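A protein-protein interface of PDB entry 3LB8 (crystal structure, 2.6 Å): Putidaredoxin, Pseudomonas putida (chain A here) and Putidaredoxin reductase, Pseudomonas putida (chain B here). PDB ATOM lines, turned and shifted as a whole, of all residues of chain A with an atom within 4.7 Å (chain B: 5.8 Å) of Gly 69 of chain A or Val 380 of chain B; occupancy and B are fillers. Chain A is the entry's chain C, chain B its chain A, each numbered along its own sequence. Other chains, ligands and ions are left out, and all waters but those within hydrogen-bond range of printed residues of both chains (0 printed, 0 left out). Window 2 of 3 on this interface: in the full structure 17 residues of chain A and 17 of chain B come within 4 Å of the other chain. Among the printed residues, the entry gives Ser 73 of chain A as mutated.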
ATOM      1  N   GLU A  65      17.269  11.565  -5.003  1.00  0.00           N
ATOM      2  CA  GLU A  65      16.256  10.987  -4.130  1.00  0.00           C
ATOM      3  C   GLU A  65      16.313  11.524  -2.701  1.00  0.00           C
ATOM      4  O   GLU A  65      15.275  11.732  -2.064  1.00  0.00           O
ATOM      5  CB  GLU A  65      16.409   9.476  -4.128  1.00  0.00           C
ATOM      6  CG  GLU A  65      16.414   8.889  -5.521  1.00  0.00           C
ATOM      7  CD  GLU A  65      16.984   7.490  -5.544  1.00  0.00           C
ATOM      8  OE1 GLU A  65      16.422   6.610  -4.855  1.00  0.00           O
ATOM      9  OE2 GLU A  65      17.993   7.268  -6.249  1.00  0.00           O
ATOM     10  N   ARG A  66      17.525  11.736  -2.197  1.00  0.00           N
ATOM     11  CA  ARG A  66      17.711  12.267  -0.852  1.00  0.00           C
ATOM     12  C   ARG A  66      16.895  13.544  -0.745  1.00  0.00           C
ATOM     13  O   ARG A  66      15.962  13.641   0.058  1.00  0.00           O
ATOM     14  CB  ARG A  66      19.184  12.605  -0.619  1.00  0.00           C
ATOM     15  CG  ARG A  66      19.848  11.866   0.526  1.00  0.00           C
ATOM     16  CD  ARG A  66      20.076  12.746   1.745  1.00  0.00           C
ATOM     17  NE  ARG A  66      21.351  12.403   2.375  1.00  0.00           N
ATOM     18  CZ  ARG A  66      21.686  12.683   3.633  1.00  0.00           C
ATOM     19  NH1 ARG A  66      20.844  13.317   4.435  1.00  0.00           N
ATOM     20  NH2 ARG A  66      22.879  12.326   4.093  1.00  0.00           N
ATOM     21  N   GLU A  67      17.263  14.519  -1.581  1.00  0.00           N
ATOM     22  CA  GLU A  67      16.606  15.824  -1.609  1.00  0.00           C
ATOM     23  C   GLU A  67      15.115  15.745  -1.894  1.00  0.00           C
ATOM     24  O   GLU A  67      14.312  16.384  -1.210  1.00  0.00           O
ATOM     25  CB  GLU A  67      17.253  16.731  -2.649  1.00  0.00           C
ATOM     26  CG  GLU A  67      16.809  18.167  -2.500  1.00  0.00           C
ATOM     27  CD  GLU A  67      17.317  19.062  -3.603  1.00  0.00           C
ATOM     28  OE1 GLU A  67      18.529  19.016  -3.902  1.00  0.00           O
ATOM     29  OE2 GLU A  67      16.494  19.815  -4.169  1.00  0.00           O
ATOM     30  N   ILE A  68      14.747  14.983  -2.916  1.00  0.00           N
ATOM     31  CA  ILE A  68      13.344  14.832  -3.252  1.00  0.00           C
ATOM     32  C   ILE A  68      12.614  14.363  -1.994  1.00  0.00           C
ATOM     33  O   ILE A  68      11.545  14.883  -1.651  1.00  0.00           O
ATOM     34  CB  ILE A  68      13.145  13.793  -4.370  1.00  0.00           C
ATOM     35  CG1 ILE A  68      13.874  14.245  -5.639  1.00  0.00           C
ATOM     36  CG2 ILE A  68      11.658  13.606  -4.639  1.00  0.00           C
ATOM     37  CD1 ILE A  68      13.852  13.223  -6.765  1.00  0.00           C
ATOM     38  N   GLY A  69      13.208  13.388  -1.302  1.00  0.00           N
ATOM     39  CA  GLY A  69      12.617  12.857  -0.083  1.00  0.00           C
ATOM     40  C   GLY A  69      12.485  13.935   0.975  1.00  0.00           C
ATOM     41  O   GLY A  69      11.488  13.994   1.689  1.00  0.00           O
ATOM     42  N   MET A  70      13.507  14.783   1.077  1.00  0.00           N
ATOM     43  CA  MET A  70      13.510  15.880   2.034  1.00  0.00           C
ATOM     44  C   MET A  70      12.489  16.929   1.618  1.00  0.00           C
ATOM     45  O   MET A  70      11.582  17.270   2.382  1.00  0.00           O
ATOM     46  CB  MET A  70      14.895  16.526   2.104  1.00  0.00           C
ATOM     47  CG  MET A  70      15.984  15.633   2.682  1.00  0.00           C
ATOM     48  SD  MET A  70      15.751  15.168   4.434  1.00  0.00           S
ATOM     49  CE  MET A  70      15.169  13.477   4.220  1.00  0.00           C
ATOM     50  N   LEU A  71      12.649  17.439   0.397  1.00  0.00           N
ATOM     51  CA  LEU A  71      11.771  18.461  -0.173  1.00  0.00           C
ATOM     52  C   LEU A  71      10.306  18.287   0.148  1.00  0.00           C
ATOM     53  O   LEU A  71       9.598  19.247   0.409  1.00  0.00           O
ATOM     54  CB  LEU A  71      11.954  18.517  -1.691  1.00  0.00           C
ATOM     55  CG  LEU A  71      13.307  19.064  -2.124  1.00  0.00           C
ATOM     56  CD1 LEU A  71      13.516  18.896  -3.635  1.00  0.00           C
ATOM     57  CD2 LEU A  71      13.397  20.534  -1.691  1.00  0.00           C
ATOM     58  N   GLU A  72       9.874  17.050   0.162  1.00  0.00           N
ATOM     59  CA  GLU A  72       8.524  16.714   0.414  1.00  0.00           C
ATOM     60  C   GLU A  72       7.984  17.247   1.727  1.00  0.00           C
ATOM     61  O   GLU A  72       6.820  17.571   1.886  1.00  0.00           O
ATOM     62  CB  GLU A  72       8.461  15.243   0.341  1.00  0.00           C
ATOM     63  CG  GLU A  72       7.192  14.865  -0.250  1.00  0.00           C
ATOM     64  CD  GLU A  72       6.764  13.539   0.327  1.00  0.00           C
ATOM     65  OE1 GLU A  72       5.933  12.790  -0.262  1.00  0.00           O
ATOM     66  OE2 GLU A  72       7.279  13.321   1.438  1.00  0.00           O
ATOM     67  N   SER A  73       8.913  17.357   2.683  1.00  0.00           N
ATOM     68  CA  SER A  73       8.557  17.846   4.013  1.00  0.00           C
ATOM     69  C   SER A  73       8.599  19.354   4.187  1.00  0.00           C
ATOM     70  O   SER A  73       8.193  19.855   5.236  1.00  0.00           O
ATOM     71  CB  SER A  73       9.462  17.194   5.085  1.00  0.00           C
ATOM     72  OG  SER A  73       9.302  15.784   5.060  1.00  0.00           O
ATOM     73  N   ARG B 378      19.306   6.583   7.008  1.00  0.00           N
ATOM     74  CA  ARG B 378      17.941   6.714   6.534  1.00  0.00           C
ATOM     75  C   ARG B 378      17.466   8.118   6.803  1.00  0.00           C
ATOM     76  O   ARG B 378      16.602   8.346   7.646  1.00  0.00           O
ATOM     77  CB  ARG B 378      17.036   5.718   7.233  1.00  0.00           C
ATOM     78  CG  ARG B 378      17.380   4.303   6.884  1.00  0.00           C
ATOM     79  CD  ARG B 378      16.163   3.444   7.016  1.00  0.00           C
ATOM     80  NE  ARG B 378      16.436   2.118   6.487  1.00  0.00           N
ATOM     81  CZ  ARG B 378      15.577   1.107   6.502  1.00  0.00           C
ATOM     82  NH1 ARG B 378      14.374   1.261   7.026  1.00  0.00           N
ATOM     83  NH2 ARG B 378      15.932  -0.054   5.980  1.00  0.00           N
ATOM     84  N   PRO B 379      18.020   9.084   6.061  1.00  0.00           N
ATOM     85  CA  PRO B 379      17.667  10.498   6.210  1.00  0.00           C
ATOM     86  C   PRO B 379      16.187  10.778   5.994  1.00  0.00           C
ATOM     87  O   PRO B 379      15.597  11.602   6.697  1.00  0.00           O
ATOM     88  CB  PRO B 379      18.530  11.186   5.148  1.00  0.00           C
ATOM     89  CG  PRO B 379      19.661  10.201   4.885  1.00  0.00           C
ATOM     90  CD  PRO B 379      18.937   8.892   4.922  1.00  0.00           C
ATOM     91  N   VAL B 380      15.586  10.087   5.029  1.00  0.00           N
ATOM     92  CA  VAL B 380      14.182  10.334   4.732  1.00  0.00           C
ATOM     93  C   VAL B 380      13.228   9.789   5.781  1.00  0.00           C
ATOM     94  O   VAL B 380      12.287  10.490   6.157  1.00  0.00           O
ATOM     95  CB  VAL B 380      13.766   9.795   3.342  1.00  0.00           C
ATOM     96  CG1 VAL B 380      12.302  10.131   3.095  1.00  0.00           C
ATOM     97  CG2 VAL B 380      14.658  10.393   2.244  1.00  0.00           C
ATOM     98  N   GLU B 381      13.427   8.557   6.248  1.00  0.00           N
ATOM     99  CA  GLU B 381      12.535   8.045   7.282  1.00  0.00           C
ATOM    100  C   GLU B 381      12.785   8.894   8.515  1.00  0.00           C
ATOM    101  O   GLU B 381      11.871   9.184   9.287  1.00  0.00           O
ATOM    102  CB  GLU B 381      12.819   6.585   7.602  1.00  0.00           C
ATOM    103  CG  GLU B 381      12.387   5.622   6.514  1.00  0.00           C
ATOM    104  CD  GLU B 381      12.506   4.177   6.944  1.00  0.00           C
ATOM    105  OE1 GLU B 381      13.449   3.864   7.704  1.00  0.00           O
ATOM    106  OE2 GLU B 381      11.667   3.354   6.516  1.00  0.00           O
ATOM    107  N   PHE B 382      14.033   9.306   8.689  1.00  0.00           N
ATOM    108  CA  PHE B 382      14.375  10.133   9.826  1.00  0.00           C
ATOM    109  C   PHE B 382      13.569  11.429   9.818  1.00  0.00           C
ATOM    110  O   PHE B 382      12.860  11.732  10.779  1.00  0.00           O
ATOM    111  CB  PHE B 382      15.865  10.469   9.825  1.00  0.00           C
ATOM    112  CG  PHE B 382      16.208  11.650  10.683  1.00  0.00           C
ATOM    113  CD1 PHE B 382      16.046  11.595  12.065  1.00  0.00           C
ATOM    114  CD2 PHE B 382      16.649  12.840  10.105  1.00  0.00           C
ATOM    115  CE1 PHE B 382      16.316  12.706  12.865  1.00  0.00           C
ATOM    116  CE2 PHE B 382      16.923  13.957  10.892  1.00  0.00           C
ATOM    117  CZ  PHE B 382      16.753  13.887  12.278  1.00  0.00           C
ATOM    118  N   ASN B 383      13.677  12.190   8.734  1.00  0.00           N
ATOM    119  CA  ASN B 383      12.978  13.461   8.618  1.00  0.00           C
ATOM    120  C   ASN B 383      11.459  13.314   8.760  1.00  0.00           C
ATOM    121  O   ASN B 383      10.809  14.164   9.363  1.00  0.00           O
ATOM    122  CB  ASN B 383      13.360  14.119   7.291  1.00  0.00           C
ATOM    123  CG  ASN B 383      12.875  15.554   7.180  1.00  0.00           C
ATOM    124  OD1 ASN B 383      11.974  15.853   6.388  1.00  0.00           O
ATOM    125  ND2 ASN B 383      13.473  16.454   7.963  1.00  0.00           N
ATOM    126  N   GLN B 384      10.895  12.236   8.229  1.00  0.00           N
ATOM    127  CA  GLN B 384       9.455  12.014   8.332  1.00  0.00           C
ATOM    128  C   GLN B 384       9.018  11.676   9.745  1.00  0.00           C
ATOM    129  O   GLN B 384       7.870  11.909  10.109  1.00  0.00           O
ATOM    130  CB  GLN B 384       9.017  10.873   7.433  1.00  0.00           C
ATOM    131  CG  GLN B 384       9.442  11.048   6.004  1.00  0.00           C
ATOM    132  CD  GLN B 384       9.127   9.833   5.161  1.00  0.00           C
ATOM    133  OE1 GLN B 384       9.290   8.691   5.608  1.00  0.00           O
ATOM    134  NE2 GLN B 384       8.699  10.066   3.923  1.00  0.00           N
ATOM    135  N   SER B 385       9.920  11.096  10.531  1.00  0.00           N
ATOM    136  CA  SER B 385       9.603  10.727  11.899  1.00  0.00           C
ATOM    137  C   SER B 385       9.432  11.948  12.780  1.00  0.00           C
ATOM    138  O   SER B 385       8.831  11.860  13.856  1.00  0.00           O
ATOM    139  CB  SER B 385      10.694   9.829  12.484  1.00  0.00           C
ATOM    140  OG  SER B 385      10.682   8.559  11.867  1.00  0.00           O
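The side-chain hydroxyl of Ser 73 of chain A sits at hydrogen-bond distance from the side-chain amide oxygen of Asn 383 of chain B, 3.0 Å away.
Among the printed residues, merely in contact across the chains: Met 70 of chain A with Pro 379 of chain B, Arg 66 of chain A with Pro 379 of chain B, Met 70 of chain A with Val 380 of chain B, Met 70 of chain A with Asn 383 of chain B and Gly 69 of chain A with Val 380 of chain B.
Of the printed residues of chain B, Arg 66 of chain A touches Pro 379. Of chain B, only Val 380 comes within 4 Å of Gly 69 of chain A. Of the printed residues of chain B, Met 70 of chain A touches Pro 379, Val 380 and Asn 383. Of the printed residues of chain B, Ser 73 of chain A touches Asn 383. Of the printed residues of chain A, Pro 379 of chain B touches Arg 66 (3.2 Å) and Met 70 (3.1 Å). Val 380 of chain B touches just these residues of chain A: Gly 69 and Met 70. The nearest residue of chain B that does not touch Gly 69 of chain A is Asn 383 of chain B (5.1 Å). The nearest residue of chain A that does not touch Val 380 of chain B is Arg 66 of chain A (4.1 Å). The nearest printed residue of chain A that does not touch Pro 379 of chain B is Gly 69 of chain A (6.9 Å).
Of the 9 printed residues of chain A, 4 touch a printed residue of chain B. Printed residues of chain A that touch a printed residue of chain B: Arg 66, Gly 69, Met 70 and Ser 73. Hydrophobic or aromatic side chains of chain A that line the printed part of chain B: Met 70. Of the 8 printed residues of chain B, 3 touch a printed residue of chain A. Hydrophobic or aromatic side chains of chain B within 4 Å of the printed part of chain A: Pro 379 and Val 380. Among the printed residues, 6 pairs touch across the chains. Among the printed residues, no Asp or Glu carboxylate lies within 4 Å of a Lys or Arg side-chain nitrogen of the other chain.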
